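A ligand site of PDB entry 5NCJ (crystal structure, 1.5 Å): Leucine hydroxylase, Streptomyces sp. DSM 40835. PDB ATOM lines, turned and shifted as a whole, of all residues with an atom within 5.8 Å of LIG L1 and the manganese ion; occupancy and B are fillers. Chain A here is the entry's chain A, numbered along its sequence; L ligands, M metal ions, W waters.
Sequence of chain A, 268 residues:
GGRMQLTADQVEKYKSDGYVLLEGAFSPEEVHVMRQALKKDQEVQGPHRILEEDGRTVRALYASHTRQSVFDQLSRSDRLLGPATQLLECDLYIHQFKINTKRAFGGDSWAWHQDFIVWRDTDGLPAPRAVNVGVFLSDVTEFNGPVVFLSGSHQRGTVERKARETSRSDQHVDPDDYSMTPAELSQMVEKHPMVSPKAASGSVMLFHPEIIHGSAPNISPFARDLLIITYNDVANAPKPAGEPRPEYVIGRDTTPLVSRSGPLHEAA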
ATOM      1  N   TYR A  62      -5.713  -0.182  -2.665  1.00  0.00           N
ATOM      2  CA  TYR A  62      -5.653  -0.325  -4.106  1.00  0.00           C
ATOM      3  C   TYR A  62      -4.775  -1.498  -4.524  1.00  0.00           C
ATOM      4  O   TYR A  62      -3.730  -1.761  -3.916  1.00  0.00           O
ATOM      5  CB  TYR A  62      -5.149   0.962  -4.777  1.00  0.00           C
ATOM      6  CG  TYR A  62      -6.233   2.009  -4.815  1.00  0.00           C
ATOM      7  CD1 TYR A  62      -7.171   2.031  -5.841  1.00  0.00           C
ATOM      8  CD2 TYR A  62      -6.356   2.943  -3.787  1.00  0.00           C
ATOM      9  CE1 TYR A  62      -8.182   2.978  -5.852  1.00  0.00           C
ATOM     10  CE2 TYR A  62      -7.364   3.878  -3.805  1.00  0.00           C
ATOM     11  CZ  TYR A  62      -8.287   3.890  -4.835  1.00  0.00           C
ATOM     12  OH  TYR A  62      -9.284   4.809  -4.879  1.00  0.00           O
ATOM     13  N   GLN A  96      -9.388  -0.492 -12.436  1.00  0.00           N
ATOM     14  CA  GLN A  96      -9.163  -0.146 -11.037  1.00  0.00           C
ATOM     15  C   GLN A  96      -9.602  -1.313 -10.165  1.00  0.00           C
ATOM     16  O   GLN A  96     -10.617  -1.955 -10.432  1.00  0.00           O
ATOM     17  CB  GLN A  96      -9.924   1.137 -10.678  1.00  0.00           C
ATOM     18  CG  GLN A  96      -9.776   1.611  -9.237  1.00  0.00           C
ATOM     19  CD  GLN A  96     -10.177   3.056  -9.069  1.00  0.00           C
ATOM     20  OE1 GLN A  96     -11.236   3.351  -8.531  1.00  0.00           O
ATOM     21  NE2 GLN A  96      -9.330   3.962  -9.535  1.00  0.00           N
ATOM     22  N   LYS A  98     -10.074  -1.850  -6.033  1.00  0.00           N
ATOM     23  CA  LYS A  98     -10.027  -1.233  -4.724  1.00  0.00           C
ATOM     24  C   LYS A  98     -10.861  -2.028  -3.748  1.00  0.00           C
ATOM     25  O   LYS A  98     -11.821  -2.699  -4.109  1.00  0.00           O
ATOM     26  CB  LYS A  98     -10.496   0.227  -4.756  1.00  0.00           C
ATOM     27  CG  LYS A  98     -11.914   0.440  -5.300  1.00  0.00           C
ATOM     28  CD  LYS A  98     -12.280   1.941  -5.208  1.00  0.00           C
ATOM     29  CE  LYS A  98     -13.589   2.262  -5.857  1.00  0.00           C
ATOM     30  NZ  LYS A  98     -13.521   2.134  -7.364  1.00  0.00           N
ATOM     31  N   ASN A 100     -12.772  -0.845  -0.295  1.00  0.00           N
ATOM     32  CA  ASN A 100     -13.156   0.256   0.594  1.00  0.00           C
ATOM     33  C   ASN A 100     -13.579  -0.368   1.925  1.00  0.00           C
ATOM     34  O   ASN A 100     -14.679  -0.927   2.053  1.00  0.00           O
ATOM     35  CB  ASN A 100     -14.254   1.116  -0.014  1.00  0.00           C
ATOM     36  CG  ASN A 100     -13.751   1.965  -1.183  1.00  0.00           C
ATOM     37  OD1 ASN A 100     -12.552   2.117  -1.403  1.00  0.00           O
ATOM     38  ND2 ASN A 100     -14.687   2.575  -1.895  1.00  0.00           N
ATOM     39  N   TRP A 110     -18.595   8.054   2.008  1.00  0.00           N
ATOM     40  CA  TRP A 110     -18.119   8.303   0.648  1.00  0.00           C
ATOM     41  C   TRP A 110     -19.103   9.265  -0.007  1.00  0.00           C
ATOM     42  O   TRP A 110     -20.312   9.007  -0.038  1.00  0.00           O
ATOM     43  CB  TRP A 110     -17.991   7.002  -0.156  1.00  0.00           C
ATOM     44  CG  TRP A 110     -16.875   6.097   0.349  1.00  0.00           C
ATOM     45  CD1 TRP A 110     -16.988   5.047   1.234  1.00  0.00           C
ATOM     46  CD2 TRP A 110     -15.483   6.180   0.028  1.00  0.00           C
ATOM     47  NE1 TRP A 110     -15.760   4.477   1.465  1.00  0.00           N
ATOM     48  CE2 TRP A 110     -14.823   5.158   0.734  1.00  0.00           C
ATOM     49  CE3 TRP A 110     -14.748   7.009  -0.818  1.00  0.00           C
ATOM     50  CZ2 TRP A 110     -13.452   4.938   0.614  1.00  0.00           C
ATOM     51  CZ3 TRP A 110     -13.392   6.816  -0.906  1.00  0.00           C
ATOM     52  CH2 TRP A 110     -12.752   5.774  -0.192  1.00  0.00           C
ATOM     53  N   HIS A 113     -21.365  10.886  -5.855  1.00  0.00           N
ATOM     54  CA  HIS A 113     -20.566  11.168  -7.045  1.00  0.00           C
ATOM     55  C   HIS A 113     -20.951  10.222  -8.172  1.00  0.00           C
ATOM     56  O   HIS A 113     -21.633   9.203  -7.970  1.00  0.00           O
ATOM     57  CB  HIS A 113     -19.072  11.033  -6.751  1.00  0.00           C
ATOM     58  CG  HIS A 113     -18.650   9.631  -6.434  1.00  0.00           C
ATOM     59  ND1 HIS A 113     -18.973   9.010  -5.252  1.00  0.00           N
ATOM     60  CD2 HIS A 113     -17.946   8.717  -7.155  1.00  0.00           C
ATOM     61  CE1 HIS A 113     -18.481   7.772  -5.250  1.00  0.00           C
ATOM     62  NE2 HIS A 113     -17.856   7.572  -6.394  1.00  0.00           N
ATOM     63  N   GLN A 114     -20.475  10.562  -9.379  1.00  0.00           N
ATOM     64  CA  GLN A 114     -20.326   9.638 -10.498  1.00  0.00           C
ATOM     65  C   GLN A 114     -18.854   9.292 -10.663  1.00  0.00           C
ATOM     66  O   GLN A 114     -17.986  10.136 -10.481  1.00  0.00           O
ATOM     67  CB  GLN A 114     -20.824  10.263 -11.806  1.00  0.00           C
ATOM     68  CG  GLN A 114     -22.275  10.743 -11.815  1.00  0.00           C
ATOM     69  CD  GLN A 114     -22.639  11.426 -13.110  1.00  0.00           C
ATOM     70  OE1 GLN A 114     -22.026  12.442 -13.499  1.00  0.00           O
ATOM     71  NE2 GLN A 114     -23.617  10.872 -13.818  1.00  0.00           N
ATOM     72  N   ASP A 115     -18.576   8.039 -11.090  1.00  0.00           N
ATOM     73  CA  ASP A 115     -17.197   7.621 -11.294  1.00  0.00           C
ATOM     74  C   ASP A 115     -16.614   8.167 -12.584  1.00  0.00           C
ATOM     75  O   ASP A 115     -15.460   8.602 -12.612  1.00  0.00           O
ATOM     76  CB  ASP A 115     -17.076   6.098 -11.337  1.00  0.00           C
ATOM     77  CG  ASP A 115     -17.252   5.448  -9.999  1.00  0.00           C
ATOM     78  OD1 ASP A 115     -17.144   6.119  -8.951  1.00  0.00           O
ATOM     79  OD2 ASP A 115     -17.483   4.232 -10.006  1.00  0.00           O
ATOM     80  N   VAL A 118     -14.618  11.506 -13.164  1.00  0.00           N
ATOM     81  CA  VAL A 118     -13.306  11.538 -12.516  1.00  0.00           C
ATOM     82  C   VAL A 118     -12.248  10.940 -13.431  1.00  0.00           C
ATOM     83  O   VAL A 118     -11.161  11.494 -13.617  1.00  0.00           O
ATOM     84  CB  VAL A 118     -13.336  10.787 -11.181  1.00  0.00           C
ATOM     85  CG1 VAL A 118     -11.943  10.792 -10.543  1.00  0.00           C
ATOM     86  CG2 VAL A 118     -14.380  11.390 -10.251  1.00  0.00           C
ATOM     87  N   TRP A 119     -12.550   9.766 -13.981  1.00  0.00           N
ATOM     88  CA  TRP A 119     -11.570   9.101 -14.844  1.00  0.00           C
ATOM     89  C   TRP A 119     -11.420   9.823 -16.174  1.00  0.00           C
ATOM     90  O   TRP A 119     -10.314   9.874 -16.718  1.00  0.00           O
ATOM     91  CB  TRP A 119     -11.988   7.644 -15.037  1.00  0.00           C
ATOM     92  CG  TRP A 119     -12.003   6.866 -13.733  1.00  0.00           C
ATOM     93  CD1 TRP A 119     -11.145   7.017 -12.687  1.00  0.00           C
ATOM     94  CD2 TRP A 119     -12.931   5.829 -13.342  1.00  0.00           C
ATOM     95  NE1 TRP A 119     -11.468   6.155 -11.678  1.00  0.00           N
ATOM     96  CE2 TRP A 119     -12.546   5.397 -12.051  1.00  0.00           C
ATOM     97  CE3 TRP A 119     -14.033   5.224 -13.963  1.00  0.00           C
ATOM     98  CZ2 TRP A 119     -13.232   4.397 -11.367  1.00  0.00           C
ATOM     99  CZ3 TRP A 119     -14.708   4.206 -13.271  1.00  0.00           C
ATOM    100  CH2 TRP A 119     -14.304   3.804 -11.991  1.00  0.00           C
ATOM    101  N   ASP A 123      -7.804  11.150 -15.947  1.00  0.00           N
ATOM    102  CA  ASP A 123      -7.020  10.101 -16.577  1.00  0.00           C
ATOM    103  C   ASP A 123      -7.225  10.000 -18.077  1.00  0.00           C
ATOM    104  O   ASP A 123      -6.524   9.217 -18.730  1.00  0.00           O
ATOM    105  CB  ASP A 123      -7.351   8.755 -15.919  1.00  0.00           C
ATOM    106  CG  ASP A 123      -7.209   8.815 -14.432  1.00  0.00           C
ATOM    107  OD1 ASP A 123      -6.068   9.080 -13.983  1.00  0.00           O
ATOM    108  OD2 ASP A 123      -8.233   8.626 -13.732  1.00  0.00           O
ATOM    109  N   ASN A 132     -18.481  -1.418 -12.896  1.00  0.00           N
ATOM    110  CA  ASN A 132     -18.000  -1.651 -11.550  1.00  0.00           C
ATOM    111  C   ASN A 132     -18.607  -2.943 -11.023  1.00  0.00           C
ATOM    112  O   ASN A 132     -19.816  -3.136 -11.123  1.00  0.00           O
ATOM    113  CB  ASN A 132     -18.383  -0.490 -10.631  1.00  0.00           C
ATOM    114  CG  ASN A 132     -17.735   0.820 -11.062  1.00  0.00           C
ATOM    115  OD1 ASN A 132     -16.525   0.893 -11.271  1.00  0.00           O
ATOM    116  ND2 ASN A 132     -18.554   1.857 -11.199  1.00  0.00           N
ATOM    117  N   HIS A 172      -5.149   9.233  -4.039  1.00  0.00           N
ATOM    118  CA  HIS A 172      -6.192   8.898  -5.002  1.00  0.00           C
ATOM    119  C   HIS A 172      -7.115  10.110  -5.106  1.00  0.00           C
ATOM    120  O   HIS A 172      -6.892  11.127  -4.451  1.00  0.00           O
ATOM    121  CB  HIS A 172      -6.962   7.628  -4.612  1.00  0.00           C
ATOM    122  CG  HIS A 172      -7.831   7.761  -3.398  1.00  0.00           C
ATOM    123  ND1 HIS A 172      -8.933   6.961  -3.196  1.00  0.00           N
ATOM    124  CD2 HIS A 172      -7.758   8.571  -2.318  1.00  0.00           C
ATOM    125  CE1 HIS A 172      -9.513   7.286  -2.064  1.00  0.00           C
ATOM    126  NE2 HIS A 172      -8.826   8.260  -1.508  1.00  0.00           N
ATOM    127  N   VAL A 173      -8.133  10.008  -5.938  1.00  0.00           N
ATOM    128  CA  VAL A 173      -9.146  11.056  -6.038  1.00  0.00           C
ATOM    129  C   VAL A 173     -10.301  10.621  -5.156  1.00  0.00           C
ATOM    130  O   VAL A 173     -11.088   9.741  -5.508  1.00  0.00           O
ATOM    131  CB  VAL A 173      -9.607  11.296  -7.486  1.00  0.00           C
ATOM    132  CG1 VAL A 173     -10.715  12.352  -7.523  1.00  0.00           C
ATOM    133  CG2 VAL A 173      -8.445  11.751  -8.338  1.00  0.00           C
ATOM    134  N   ASP A 174     -10.393  11.215  -3.966  1.00  0.00           N
ATOM    135  CA  ASP A 174     -11.568  10.993  -3.138  1.00  0.00           C
ATOM    136  C   ASP A 174     -12.774  11.601  -3.836  1.00  0.00           C
ATOM    137  O   ASP A 174     -12.671  12.706  -4.379  1.00  0.00           O
ATOM    138  CB  ASP A 174     -11.354  11.632  -1.765  1.00  0.00           C
ATOM    139  CG  ASP A 174     -12.443  11.249  -0.784  1.00  0.00           C
ATOM    140  OD1 ASP A 174     -13.571  11.748  -0.922  1.00  0.00           O
ATOM    141  OD2 ASP A 174     -12.163  10.416   0.115  1.00  0.00           O
ATOM    142  N   PRO A 175     -13.925  10.917  -3.850  1.00  0.00           N
ATOM    143  CA  PRO A 175     -15.105  11.462  -4.525  1.00  0.00           C
ATOM    144  C   PRO A 175     -15.536  12.835  -4.016  1.00  0.00           C
ATOM    145  O   PRO A 175     -16.247  13.542  -4.757  1.00  0.00           O
ATOM    146  CB  PRO A 175     -16.179  10.399  -4.266  1.00  0.00           C
ATOM    147  CG  PRO A 175     -15.658   9.527  -3.165  1.00  0.00           C
ATOM    148  CD  PRO A 175     -14.156   9.589  -3.281  1.00  0.00           C
ATOM    149  N   PHE A 207     -22.503  -2.275 -11.129  1.00  0.00           N
ATOM    150  CA  PHE A 207     -23.100  -0.962 -11.282  1.00  0.00           C
ATOM    151  C   PHE A 207     -22.345  -0.097 -12.280  1.00  0.00           C
ATOM    152  O   PHE A 207     -21.149  -0.261 -12.517  1.00  0.00           O
ATOM    153  CB  PHE A 207     -23.266  -0.240  -9.930  1.00  0.00           C
ATOM    154  CG  PHE A 207     -21.985   0.039  -9.153  1.00  0.00           C
ATOM    155  CD1 PHE A 207     -21.381  -0.952  -8.387  1.00  0.00           C
ATOM    156  CD2 PHE A 207     -21.444   1.313  -9.115  1.00  0.00           C
ATOM    157  CE1 PHE A 207     -20.255  -0.680  -7.619  1.00  0.00           C
ATOM    158  CE2 PHE A 207     -20.309   1.586  -8.345  1.00  0.00           C
ATOM    159  CZ  PHE A 207     -19.727   0.587  -7.606  1.00  0.00           C
ATOM    160  N   HIS A 213     -23.856   7.559  -6.794  1.00  0.00           N
ATOM    161  CA  HIS A 213     -23.775   6.679  -5.641  1.00  0.00           C
ATOM    162  C   HIS A 213     -22.969   7.364  -4.557  1.00  0.00           C
ATOM    163  O   HIS A 213     -22.187   8.283  -4.822  1.00  0.00           O
ATOM    164  CB  HIS A 213     -23.188   5.324  -6.012  1.00  0.00           C
ATOM    165  CG  HIS A 213     -21.814   5.378  -6.603  1.00  0.00           C
ATOM    166  ND1 HIS A 213     -21.563   5.845  -7.874  1.00  0.00           N
ATOM    167  CD2 HIS A 213     -20.619   4.929  -6.129  1.00  0.00           C
ATOM    168  CE1 HIS A 213     -20.271   5.745  -8.146  1.00  0.00           C
ATOM    169  NE2 HIS A 213     -19.673   5.197  -7.101  1.00  0.00           N
ATOM    170  N   ARG A 245      -1.381   8.742 -13.737  1.00  0.00           N
ATOM    171  CA  ARG A 245      -1.405   8.391 -12.337  1.00  0.00           C
ATOM    172  C   ARG A 245      -0.808   7.005 -12.146  1.00  0.00           C
ATOM    173  O   ARG A 245      -0.600   6.261 -13.110  1.00  0.00           O
ATOM    174  CB  ARG A 245      -2.836   8.452 -11.802  1.00  0.00           C
ATOM    175  CG  ARG A 245      -3.364   9.868 -11.618  1.00  0.00           C
ATOM    176  CD  ARG A 245      -4.477   9.890 -10.584  1.00  0.00           C
ATOM    177  NE  ARG A 245      -5.707   9.279 -11.097  1.00  0.00           N
ATOM    178  CZ  ARG A 245      -6.677   8.790 -10.333  1.00  0.00           C
ATOM    179  NH1 ARG A 245      -6.570   8.786  -9.006  1.00  0.00           N
ATOM    180  NH2 ARG A 245      -7.762   8.311 -10.910  1.00  0.00           N
ATOM    181  N   VAL A 249      -3.675   2.771  -9.055  1.00  0.00           N
ATOM    182  CA  VAL A 249      -5.010   3.359  -9.090  1.00  0.00           C
ATOM    183  C   VAL A 249      -5.610   3.286 -10.496  1.00  0.00           C
ATOM    184  O   VAL A 249      -6.821   3.104 -10.631  1.00  0.00           O
ATOM    185  CB  VAL A 249      -5.017   4.801  -8.512  1.00  0.00           C
ATOM    186  CG1 VAL A 249      -4.048   5.722  -9.209  1.00  0.00           C
ATOM    187  CG2 VAL A 249      -6.415   5.392  -8.516  1.00  0.00           C
ATOM    188  N   ILE A 250      -4.792   3.327 -11.539  1.00  0.00           N
ATOM    189  CA  ILE A 250      -5.301   3.299 -12.923  1.00  0.00           C
ATOM    190  C   ILE A 250      -4.528   2.238 -13.717  1.00  0.00           C
ATOM    191  O   ILE A 250      -3.333   2.396 -13.994  1.00  0.00           O
ATOM    192  CB  ILE A 250      -5.212   4.677 -13.608  1.00  0.00           C
ATOM    193  CG1 ILE A 250      -6.098   5.710 -12.880  1.00  0.00           C
ATOM    194  CG2 ILE A 250      -5.619   4.594 -15.085  1.00  0.00           C
ATOM    195  CD1 ILE A 250      -7.628   5.454 -12.905  1.00  0.00           C
HETATM  196  N1  LIG L   1     -10.906   6.997  -6.017  1.00  0.00           N
HETATM  197  C1  LIG L   1     -11.056   6.763  -7.447  1.00  0.00           C
HETATM  198  C2  LIG L   1      -9.777   7.108  -8.201  1.00  0.00           C
HETATM  199  O1  LIG L   1      -9.698   6.863  -9.440  1.00  0.00           O
HETATM  200  C3  LIG L   1     -12.217   7.588  -8.004  1.00  0.00           C
HETATM  201  C4  LIG L   1     -13.527   7.346  -7.240  1.00  0.00           C
HETATM  202  O2  LIG L   1     -15.227   5.673  -6.741  1.00  0.00           O
HETATM  203  C5  LIG L   1     -14.059   5.943  -7.506  1.00  0.00           C
HETATM  204  C6  LIG L   1     -14.538   8.383  -7.715  1.00  0.00           C
HETATM  205  O3  LIG L   1      -8.834   7.647  -7.578  1.00  0.00           O
HETATM  206  C1  LG2 L   2     -18.288   3.025  -1.092  1.00  0.00           C
HETATM  207  O1  LG2 L   2     -17.374   2.234  -0.716  1.00  0.00           O
HETATM  208  O2  LG2 L   2     -19.295   3.113  -0.327  1.00  0.00           O
HETATM  209  C2  LG2 L   2     -18.199   3.792  -2.388  1.00  0.00           C
HETATM  210  C3  LG2 L   2     -17.908   2.843  -3.538  1.00  0.00           C
HETATM  211  C4  LG2 L   2     -17.560   3.558  -4.851  1.00  0.00           C
HETATM  212  O3  LG2 L   2     -17.243   4.765  -4.909  1.00  0.00           O
HETATM  213  O4  LG2 L   2     -17.592   2.919  -5.922  1.00  0.00           O
HETATM  214 MN    MN M   1     -17.426   5.442  -6.985  1.00  0.00          MN
HETATM  215  O   HOH W   1     -16.350   2.868  -7.933  1.00  0.00           O
HETATM  216  O   HOH W   2     -12.654   5.774  -4.422  1.00  0.00           O
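The side-chain hydroxyl (OH) of Tyr 62 sits at hydrogen-bond distance from a ring nitrogen (ND1) of His 172.
The side-chain amide nitrogen (NE2) of Gln 96 lies within hydrogen-bond range of the backbone carbonyl oxygen (O) of Val 249 (2.9 Å).
The guanidinium group (NH2) of Arg 245 is in salt-bridge range of the side-chain carboxylate (OD2) of Asp 123.
The side-chain amide oxygen (OE1) of Gln 96 is in hydrogen-bond range of the side-chain amino group (NZ) of Lys 98, at 2.8 Å.
OD2 of Asp 115 sits at hydrogen-bond distance from ND2 of Asn 132 (2.9 Å).
Water W1 lies within hydrogen-bond range of the side-chain carboxylate (OD2) of Asp 115 (2.7 Å) and the side-chain amino group (NZ) of Lys 98 (3.0 Å).
The manganese ion is bound by OD1 of Asp 115 (2.1 Å), O3 of LG2 L2 (2.2 Å), O2 of LIG L1 (2.2 Å), NE2 of His 113 (2.3 Å) and NE2 of His 213 (2.3 Å).
The manganese ion has five donor atoms within binding distance.
Slightly farther from the manganese ion lies an oxygen (O4) of LG2 L2 (2.7 Å).
Slightly farther from the manganese ion lies water W1 (2.9 Å).
Within 4 Å of the manganese ion: His 113, Asp 115 and His 213.
The nearest printed residue that does not touch the manganese ion is Phe 207 (5.0 Å).
Lys 98 touches LIG L1.
CG2 of Val 118 touches C6 of LIG L1 (3.9 Å).
Val 249 touches LIG L1 (CG2 to O3, 3.4 Å).
Of the 21 residues printed, 11 come within 4 Å of LIG L1.
The nearest printed residue that does not touch LIG L1 is Ile 250 (4.3 Å).
NE2 of Gln 96 is in hydrogen-bond range of O1 of LIG L1 (2.9 Å).
O1 of LIG L1 sits at hydrogen-bond distance from NE1 of Trp 119, at 2.9 Å.
A ring nitrogen (ND1) of His 172 sits at hydrogen-bond distance from a nitrogen (N1) of LIG L1, 3.4 Å away.
The backbone NH (N) of Val 173 sits at hydrogen-bond distance from an oxygen (O3) of LIG L1.
NH2 of Arg 245 lies within salt-bridge range of O1 of LIG L1.
N1 of LIG L1 is in hydrogen-bond range of O of Val 173.
OH of Tyr 62 lies within hydrogen-bond range of N1 of LIG L1 (3.0 Å).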
